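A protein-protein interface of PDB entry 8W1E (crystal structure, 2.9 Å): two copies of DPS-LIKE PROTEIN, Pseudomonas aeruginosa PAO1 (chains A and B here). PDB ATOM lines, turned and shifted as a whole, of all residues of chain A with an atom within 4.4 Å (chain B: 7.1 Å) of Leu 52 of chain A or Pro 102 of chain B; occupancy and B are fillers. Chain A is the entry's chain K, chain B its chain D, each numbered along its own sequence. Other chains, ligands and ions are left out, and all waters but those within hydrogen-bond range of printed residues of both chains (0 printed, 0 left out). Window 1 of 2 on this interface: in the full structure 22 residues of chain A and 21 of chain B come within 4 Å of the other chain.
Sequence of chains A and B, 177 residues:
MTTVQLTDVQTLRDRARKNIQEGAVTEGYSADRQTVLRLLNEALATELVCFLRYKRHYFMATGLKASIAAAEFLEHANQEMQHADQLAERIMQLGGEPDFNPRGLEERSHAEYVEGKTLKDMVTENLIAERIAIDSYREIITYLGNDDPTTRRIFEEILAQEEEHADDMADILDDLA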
ATOM      1  N   LEU A  48      14.900 -24.602  16.619  1.00  0.00           N
ATOM      2  CA  LEU A  48      13.982 -23.671  15.968  1.00  0.00           C
ATOM      3  C   LEU A  48      14.514 -22.243  16.030  1.00  0.00           C
ATOM      4  O   LEU A  48      14.476 -21.514  15.030  1.00  0.00           O
ATOM      5  CB  LEU A  48      12.597 -23.753  16.608  1.00  0.00           C
ATOM      6  CG  LEU A  48      11.890 -25.085  16.367  1.00  0.00           C
ATOM      7  CD1 LEU A  48      10.559 -25.163  17.096  1.00  0.00           C
ATOM      8  CD2 LEU A  48      11.705 -25.318  14.874  1.00  0.00           C
ATOM      9  N   VAL A  49      15.032 -21.833  17.193  1.00  0.00           N
ATOM     10  CA  VAL A  49      15.649 -20.514  17.325  1.00  0.00           C
ATOM     11  C   VAL A  49      16.871 -20.394  16.412  1.00  0.00           C
ATOM     12  O   VAL A  49      17.001 -19.427  15.651  1.00  0.00           O
ATOM     13  CB  VAL A  49      16.012 -20.248  18.797  1.00  0.00           C
ATOM     14  CG1 VAL A  49      16.950 -19.073  18.935  1.00  0.00           C
ATOM     15  CG2 VAL A  49      14.757 -19.980  19.613  1.00  0.00           C
ATOM     16  N   CYS A  50      17.783 -21.378  16.461  1.00  0.00           N
ATOM     17  CA  CYS A  50      18.957 -21.329  15.588  1.00  0.00           C
ATOM     18  C   CYS A  50      18.547 -21.251  14.114  1.00  0.00           C
ATOM     19  O   CYS A  50      19.193 -20.559  13.321  1.00  0.00           O
ATOM     20  CB  CYS A  50      19.865 -22.543  15.831  1.00  0.00           C
ATOM     21  SG  CYS A  50      20.957 -22.487  17.307  1.00  0.00           S
ATOM     22  N   PHE A  51      17.464 -21.938  13.730  1.00  0.00           N
ATOM     23  CA  PHE A  51      16.955 -21.833  12.363  1.00  0.00           C
ATOM     24  C   PHE A  51      16.532 -20.403  12.042  1.00  0.00           C
ATOM     25  O   PHE A  51      16.870 -19.860  10.986  1.00  0.00           O
ATOM     26  CB  PHE A  51      15.771 -22.783  12.165  1.00  0.00           C
ATOM     27  CG  PHE A  51      15.012 -22.540  10.896  1.00  0.00           C
ATOM     28  CD1 PHE A  51      15.378 -23.176   9.723  1.00  0.00           C
ATOM     29  CD2 PHE A  51      13.938 -21.670  10.870  1.00  0.00           C
ATOM     30  CE1 PHE A  51      14.695 -22.945   8.555  1.00  0.00           C
ATOM     31  CE2 PHE A  51      13.247 -21.440   9.699  1.00  0.00           C
ATOM     32  CZ  PHE A  51      13.626 -22.077   8.543  1.00  0.00           C
ATOM     33  N   LEU A  52      15.755 -19.788  12.930  1.00  0.00           N
ATOM     34  CA  LEU A  52      15.288 -18.430  12.675  1.00  0.00           C
ATOM     35  C   LEU A  52      16.454 -17.441  12.617  1.00  0.00           C
ATOM     36  O   LEU A  52      16.455 -16.533  11.780  1.00  0.00           O
ATOM     37  CB  LEU A  52      14.264 -18.024  13.738  1.00  0.00           C
ATOM     38  CG  LEU A  52      12.920 -18.757  13.741  1.00  0.00           C
ATOM     39  CD1 LEU A  52      12.143 -18.447  15.018  1.00  0.00           C
ATOM     40  CD2 LEU A  52      12.116 -18.349  12.506  1.00  0.00           C
ATOM     41  N   ARG A  53      17.447 -17.580  13.504  1.00  0.00           N
ATOM     42  CA  ARG A  53      18.589 -16.662  13.467  1.00  0.00           C
ATOM     43  C   ARG A  53      19.346 -16.794  12.149  1.00  0.00           C
ATOM     44  O   ARG A  53      19.609 -15.799  11.462  1.00  0.00           O
ATOM     45  CB  ARG A  53      19.538 -16.921  14.644  1.00  0.00           C
ATOM     46  CG  ARG A  53      20.578 -15.810  14.883  1.00  0.00           C
ATOM     47  CD  ARG A  53      21.827 -16.342  15.603  1.00  0.00           C
ATOM     48  NE  ARG A  53      21.493 -17.438  16.501  1.00  0.00           N
ATOM     49  CZ  ARG A  53      21.839 -18.702  16.313  1.00  0.00           C
ATOM     50  NH1 ARG A  53      22.624 -19.062  15.315  1.00  0.00           N
ATOM     51  NH2 ARG A  53      21.383 -19.626  17.149  1.00  0.00           N
ATOM     52  N   TYR A  54      19.667 -18.033  11.758  1.00  0.00           N
ATOM     53  CA  TYR A  54      20.417 -18.249  10.527  1.00  0.00           C
ATOM     54  C   TYR A  54      19.644 -17.736   9.317  1.00  0.00           C
ATOM     55  O   TYR A  54      20.233 -17.189   8.380  1.00  0.00           O
ATOM     56  CB  TYR A  54      20.727 -19.734  10.345  1.00  0.00           C
ATOM     57  CG  TYR A  54      22.013 -20.224  10.968  1.00  0.00           C
ATOM     58  CD1 TYR A  54      23.231 -19.691  10.602  1.00  0.00           C
ATOM     59  CD2 TYR A  54      22.002 -21.258  11.898  1.00  0.00           C
ATOM     60  CE1 TYR A  54      24.401 -20.148  11.163  1.00  0.00           C
ATOM     61  CE2 TYR A  54      23.165 -21.727  12.457  1.00  0.00           C
ATOM     62  CZ  TYR A  54      24.363 -21.169  12.085  1.00  0.00           C
ATOM     63  OH  TYR A  54      25.532 -21.630  12.636  1.00  0.00           O
ATOM     64  N   LYS A  55      18.328 -17.934   9.296  1.00  0.00           N
ATOM     65  CA  LYS A  55      17.541 -17.436   8.170  1.00  0.00           C
ATOM     66  C   LYS A  55      17.630 -15.914   8.076  1.00  0.00           C
ATOM     67  O   LYS A  55      17.800 -15.358   6.983  1.00  0.00           O
ATOM     68  CB  LYS A  55      16.087 -17.899   8.303  1.00  0.00           C
ATOM     69  CG  LYS A  55      15.818 -19.289   7.714  1.00  0.00           C
ATOM     70  CD  LYS A  55      16.019 -19.321   6.200  1.00  0.00           C
ATOM     71  CE  LYS A  55      14.683 -19.498   5.472  1.00  0.00           C
ATOM     72  NZ  LYS A  55      14.674 -20.772   4.689  1.00  0.00           N
ATOM     73  N   ARG A  56      17.529 -15.228   9.219  1.00  0.00           N
ATOM     74  CA  ARG A  56      17.708 -13.779   9.240  1.00  0.00           C
ATOM     75  C   ARG A  56      19.065 -13.398   8.665  1.00  0.00           C
ATOM     76  O   ARG A  56      19.164 -12.512   7.805  1.00  0.00           O
ATOM     77  CB  ARG A  56      17.565 -13.261  10.674  1.00  0.00           C
ATOM     78  CG  ARG A  56      18.149 -11.879  10.960  1.00  0.00           C
ATOM     79  CD  ARG A  56      17.308 -10.749  10.411  1.00  0.00           C
ATOM     80  NE  ARG A  56      17.885  -9.445  10.712  1.00  0.00           N
ATOM     81  CZ  ARG A  56      17.169  -8.338  10.861  1.00  0.00           C
ATOM     82  NH1 ARG A  56      15.847  -8.357  10.796  1.00  0.00           N
ATOM     83  NH2 ARG A  56      17.790  -7.189  11.104  1.00  0.00           N
ATOM     84  N   PRO A 102       5.714 -20.416  19.350  1.00  0.00           N
ATOM     85  CA  PRO A 102       6.691 -19.316  19.339  1.00  0.00           C
ATOM     86  C   PRO A 102       6.695 -18.498  20.622  1.00  0.00           C
ATOM     87  O   PRO A 102       7.686 -17.809  20.886  1.00  0.00           O
ATOM     88  CB  PRO A 102       6.261 -18.473  18.130  1.00  0.00           C
ATOM     89  CG  PRO A 102       4.788 -18.712  18.027  1.00  0.00           C
ATOM     90  CD  PRO A 102       4.573 -20.153  18.453  1.00  0.00           C
ATOM     91  N   LEU A 105       9.554 -19.335  23.132  1.00  0.00           N
ATOM     92  CA  LEU A 105      10.528 -20.168  22.442  1.00  0.00           C
ATOM     93  C   LEU A 105      11.941 -19.856  22.923  1.00  0.00           C
ATOM     94  O   LEU A 105      12.728 -20.769  23.200  1.00  0.00           O
ATOM     95  CB  LEU A 105      10.400 -19.972  20.940  1.00  0.00           C
ATOM     96  CG  LEU A 105      11.305 -20.888  20.134  1.00  0.00           C
ATOM     97  CD1 LEU A 105      10.785 -22.314  20.168  1.00  0.00           C
ATOM     98  CD2 LEU A 105      11.419 -20.375  18.717  1.00  0.00           C
ATOM     99  N   TYR A 113      18.182 -15.648  19.625  1.00  0.00           N
ATOM    100  CA  TYR A 113      18.050 -15.009  18.319  1.00  0.00           C
ATOM    101  C   TYR A 113      18.665 -13.621  18.441  1.00  0.00           C
ATOM    102  O   TYR A 113      18.272 -12.843  19.316  1.00  0.00           O
ATOM    103  CB  TYR A 113      16.586 -14.958  17.880  1.00  0.00           C
ATOM    104  CG  TYR A 113      16.297 -14.163  16.612  1.00  0.00           C
ATOM    105  CD1 TYR A 113      16.048 -12.807  16.681  1.00  0.00           C
ATOM    106  CD2 TYR A 113      16.238 -14.767  15.361  1.00  0.00           C
ATOM    107  CE1 TYR A 113      15.765 -12.061  15.554  1.00  0.00           C
ATOM    108  CE2 TYR A 113      15.941 -14.017  14.210  1.00  0.00           C
ATOM    109  CZ  TYR A 113      15.710 -12.654  14.323  1.00  0.00           C
ATOM    110  OH  TYR A 113      15.415 -11.843  13.236  1.00  0.00           O
ATOM    111  N   LEU B  48       5.301 -17.643   9.147  1.00  0.00           N
ATOM    112  CA  LEU B  48       6.137 -18.352  10.113  1.00  0.00           C
ATOM    113  C   LEU B  48       5.298 -18.966  11.226  1.00  0.00           C
ATOM    114  O   LEU B  48       5.554 -20.098  11.652  1.00  0.00           O
ATOM    115  CB  LEU B  48       7.196 -17.415  10.685  1.00  0.00           C
ATOM    116  CG  LEU B  48       8.291 -16.975   9.720  1.00  0.00           C
ATOM    117  CD1 LEU B  48       9.203 -15.946  10.357  1.00  0.00           C
ATOM    118  CD2 LEU B  48       9.091 -18.189   9.304  1.00  0.00           C
ATOM    119  N   LEU B  52       4.794 -23.047  12.070  1.00  0.00           N
ATOM    120  CA  LEU B  52       4.951 -23.711  13.358  1.00  0.00           C
ATOM    121  C   LEU B  52       3.670 -24.432  13.758  1.00  0.00           C
ATOM    122  O   LEU B  52       3.723 -25.549  14.282  1.00  0.00           O
ATOM    123  CB  LEU B  52       5.359 -22.692  14.420  1.00  0.00           C
ATOM    124  CG  LEU B  52       6.720 -22.017  14.190  1.00  0.00           C
ATOM    125  CD1 LEU B  52       6.875 -20.842  15.156  1.00  0.00           C
ATOM    126  CD2 LEU B  52       7.868 -22.971  14.331  1.00  0.00           C
ATOM    127  N   MET B  81       6.404 -22.052   4.513  1.00  0.00           N
ATOM    128  CA  MET B  81       7.785 -21.606   4.567  1.00  0.00           C
ATOM    129  C   MET B  81       8.253 -21.079   3.214  1.00  0.00           C
ATOM    130  O   MET B  81       9.052 -20.140   3.160  1.00  0.00           O
ATOM    131  CB  MET B  81       8.678 -22.742   5.045  1.00  0.00           C
ATOM    132  CG  MET B  81      10.047 -22.286   5.497  1.00  0.00           C
ATOM    133  SD  MET B  81       9.989 -21.443   7.084  1.00  0.00           S
ATOM    134  CE  MET B  81      11.231 -20.173   6.727  1.00  0.00           C
ATOM    135  N   ASP B  99      11.829  -9.622   9.616  1.00  0.00           N
ATOM    136  CA  ASP B  99      11.881  -9.872  11.052  1.00  0.00           C
ATOM    137  C   ASP B  99      11.486 -11.312  11.354  1.00  0.00           C
ATOM    138  O   ASP B  99      10.300 -11.637  11.431  1.00  0.00           O
ATOM    139  CB  ASP B  99      10.985  -8.915  11.823  1.00  0.00           C
ATOM    140  CG  ASP B  99      11.323  -8.893  13.283  1.00  0.00           C
ATOM    141  OD1 ASP B  99      12.346  -9.557  13.624  1.00  0.00           O
ATOM    142  OD2 ASP B  99      10.595  -8.210  14.059  1.00  0.00           O
ATOM    143  N   PHE B 100      12.493 -12.160  11.554  1.00  0.00           N
ATOM    144  CA  PHE B 100      12.332 -13.548  11.951  1.00  0.00           C
ATOM    145  C   PHE B 100      12.362 -13.731  13.471  1.00  0.00           C
ATOM    146  O   PHE B 100      12.483 -14.866  13.948  1.00  0.00           O
ATOM    147  CB  PHE B 100      13.455 -14.411  11.341  1.00  0.00           C
ATOM    148  CG  PHE B 100      13.324 -14.670   9.859  1.00  0.00           C
ATOM    149  CD1 PHE B 100      12.659 -15.792   9.401  1.00  0.00           C
ATOM    150  CD2 PHE B 100      13.906 -13.817   8.934  1.00  0.00           C
ATOM    151  CE1 PHE B 100      12.555 -16.043   8.061  1.00  0.00           C
ATOM    152  CE2 PHE B 100      13.799 -14.063   7.592  1.00  0.00           C
ATOM    153  CZ  PHE B 100      13.128 -15.178   7.154  1.00  0.00           C
ATOM    154  N   ASN B 101      12.294 -12.649  14.239  1.00  0.00           N
ATOM    155  CA  ASN B 101      12.451 -12.748  15.689  1.00  0.00           C
ATOM    156  C   ASN B 101      11.281 -13.528  16.275  1.00  0.00           C
ATOM    157  O   ASN B 101      10.119 -13.163  16.039  1.00  0.00           O
ATOM    158  CB  ASN B 101      12.514 -11.357  16.321  1.00  0.00           C
ATOM    159  CG  ASN B 101      13.064 -11.373  17.746  1.00  0.00           C
ATOM    160  OD1 ASN B 101      13.009 -12.377  18.453  1.00  0.00           O
ATOM    161  ND2 ASN B 101      13.569 -10.239  18.175  1.00  0.00           N
ATOM    162  N   PRO B 102      11.528 -14.606  17.030  1.00  0.00           N
ATOM    163  CA  PRO B 102      10.406 -15.338  17.638  1.00  0.00           C
ATOM    164  C   PRO B 102       9.704 -14.544  18.730  1.00  0.00           C
ATOM    165  O   PRO B 102       8.560 -14.875  19.063  1.00  0.00           O
ATOM    166  CB  PRO B 102      11.061 -16.620  18.174  1.00  0.00           C
ATOM    167  CG  PRO B 102      12.461 -16.220  18.463  1.00  0.00           C
ATOM    168  CD  PRO B 102      12.835 -15.186  17.411  1.00  0.00           C
ATOM    169  N   ARG B 103      10.351 -13.524  19.304  1.00  0.00           N
ATOM    170  CA  ARG B 103       9.694 -12.659  20.279  1.00  0.00           C
ATOM    171  C   ARG B 103       8.668 -11.763  19.604  1.00  0.00           C
ATOM    172  O   ARG B 103       8.997 -11.031  18.666  1.00  0.00           O
ATOM    173  CB  ARG B 103      10.700 -11.782  21.016  1.00  0.00           C
ATOM    174  CG  ARG B 103      11.419 -12.466  22.109  1.00  0.00           C
ATOM    175  CD  ARG B 103      12.178 -11.482  22.973  1.00  0.00           C
ATOM    176  NE  ARG B 103      12.820 -12.245  24.034  1.00  0.00           N
ATOM    177  CZ  ARG B 103      12.181 -12.670  25.117  1.00  0.00           C
ATOM    178  NH1 ARG B 103      10.900 -12.388  25.321  1.00  0.00           N
ATOM    179  NH2 ARG B 103      12.834 -13.414  26.005  1.00  0.00           N
ATOM    180  N   GLY B 104       7.426 -11.821  20.070  1.00  0.00           N
ATOM    181  CA  GLY B 104       6.402 -11.007  19.458  1.00  0.00           C
ATOM    182  C   GLY B 104       5.970 -11.465  18.092  1.00  0.00           C
ATOM    183  O   GLY B 104       5.270 -10.725  17.397  1.00  0.00           O
ATOM    184  N   LEU B 105       6.399 -12.655  17.673  1.00  0.00           N
ATOM    185  CA  LEU B 105       5.986 -13.176  16.377  1.00  0.00           C
ATOM    186  C   LEU B 105       4.466 -13.220  16.281  1.00  0.00           C
ATOM    187  O   LEU B 105       3.884 -12.768  15.290  1.00  0.00           O
ATOM    188  CB  LEU B 105       6.613 -14.553  16.165  1.00  0.00           C
ATOM    189  CG  LEU B 105       6.406 -15.201  14.797  1.00  0.00           C
ATOM    190  CD1 LEU B 105       7.238 -14.472  13.743  1.00  0.00           C
ATOM    191  CD2 LEU B 105       6.767 -16.668  14.851  1.00  0.00           C
ATOM    192  N   GLU B 106       3.794 -13.736  17.313  1.00  0.00           N
ATOM    193  CA  GLU B 106       2.337 -13.796  17.247  1.00  0.00           C
ATOM    194  C   GLU B 106       1.729 -12.395  17.250  1.00  0.00           C
ATOM    195  O   GLU B 106       0.760 -12.136  16.526  1.00  0.00           O
ATOM    196  CB  GLU B 106       1.772 -14.642  18.392  1.00  0.00           C
ATOM    197  CG  GLU B 106       1.174 -15.975  17.894  1.00  0.00           C
ATOM    198  CD  GLU B 106       0.509 -16.826  18.973  1.00  0.00           C
ATOM    199  OE1 GLU B 106       1.140 -17.091  20.020  1.00  0.00           O
ATOM    200  OE2 GLU B 106      -0.654 -17.242  18.758  1.00  0.00           O
ATOM    201  N   ARG B 108       2.871  -9.876  15.834  1.00  0.00           N
ATOM    202  CA  ARG B 108       3.038  -9.348  14.483  1.00  0.00           C
ATOM    203  C   ARG B 108       2.169 -10.056  13.453  1.00  0.00           C
ATOM    204  O   ARG B 108       1.830  -9.462  12.424  1.00  0.00           O
ATOM    205  CB  ARG B 108       4.506  -9.481  14.040  1.00  0.00           C
ATOM    206  CG  ARG B 108       5.426  -8.361  14.473  1.00  0.00           C
ATOM    207  CD  ARG B 108       6.776  -8.870  14.940  1.00  0.00           C
ATOM    208  NE  ARG B 108       7.381  -9.765  13.968  1.00  0.00           N
ATOM    209  CZ  ARG B 108       8.386 -10.582  14.242  1.00  0.00           C
ATOM    210  NH1 ARG B 108       8.858 -10.707  15.471  1.00  0.00           N
ATOM    211  NH2 ARG B 108       8.902 -11.326  13.268  1.00  0.00           N
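Of the 12 printed residues of chain B, 7 touch a printed residue of chain A. Printed residues of chain B that touch a printed residue of chain A: Leu 52, Met 81, Asp 99, Phe 100, Asn 101, Pro 102 and Leu 105. Among the printed residues, no Asp or Glu carboxylate lies within 4 Å of a Lys or Arg side-chain nitrogen of the other chain.
N of Phe 100 of chain B is in hydrogen-bond range of OH of Tyr 113 of chain A, 3.4 Å away. The side-chain hydroxyl (OH) of Tyr 113 of chain A is in hydrogen-bond range of the backbone NH (N) of Asn 101 of chain B, 3.4 Å away.
Leu 52 of chain A touches Pro 102 of chain B, and with the chains exchanged Pro 102 of chain A touches Leu 52 of chain B. Pro 102 of chain A touches its own counterpart, Pro 102 of chain B. Pro 102 of chain A touches Leu 105 of chain B, and with the chains exchanged Leu 105 of chain A touches Pro 102 of chain B. Of the 14 pairs that touch across the chains among the printed residues, 5 have their exchanged pair printed and touching as well.
Of chain B, only Phe 100 and Pro 102 come within 4 Å of Leu 52 of chain A. Of chain A, only Leu 52 (3.8 Å), Pro 102 (3.6 Å), Leu 105 (3.8 Å) and Tyr 113 (3.7 Å) come within 4 Å of Pro 102 of chain B. Printed residues of chain B within 4 Å of Leu 105 of chain A: Pro 102. Of the printed residues of chain B, Tyr 113 of chain A touches Asp 99, Phe 100, Asn 101 and Pro 102. Of the printed residues of chain A, Leu 52 of chain B touches Pro 102 (3.9 Å). Printed residues of chain A within 4 Å of Leu 105 of chain B: Pro 102 (3.8 Å). Of the printed residues of chain B, Pro 102 of chain A touches Leu 52 (3.9 Å), Pro 102 (3.6 Å) and Leu 105 (3.8 Å). The nearest printed residue of chain A that does not touch Asp 99 of chain B is Arg 56 of chain A (4.3 Å).
The backbone NH (N) of Asn 101 of chain B lies within hydrogen-bond range of the side-chain carboxylate (OD1) of Asp 99 of chain B (3.2 Å). The guanidinium group of Arg 108 of chain B lies within salt-bridge range of the side-chain carboxylate of Asp 99 of chain B (3.4 Å). OD1 of Asn 101 of chain B lies within hydrogen-bond range of N of Arg 103 of chain B. The backbone carbonyl oxygen (O) of Asn 101 of chain B is in hydrogen-bond range of the guanidinium group (NH1) of Arg 108 of chain B (2.8 Å).
CE of Met 81 of chain B touches CZ of Phe 51 of chain A, at 3.6 Å. Leu 52 of chain A touches Phe 100 of chain B. Lys 55 of chain A touches Met 81 of chain B (CE to CE, 3.7 Å). CE1 of Phe 100 of chain B touches CB of Lys 55 of chain A, 3.997 Å away. CD2 of Phe 100 of chain B touches CA of Arg 56 of chain A, 3.8 Å away. Leu 52 of chain B touches Pro 102 of chain A (CD1 to CB, 3.9 Å). Pro 102 of chain B touches Pro 102 of chain A. CD2 of Leu 105 of chain B touches CB of Pro 102 of chain A, 3.8 Å away. Pro 102 of chain B touches Leu 105 of chain A. Asp 99 of chain B touches Tyr 113 of chain A.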
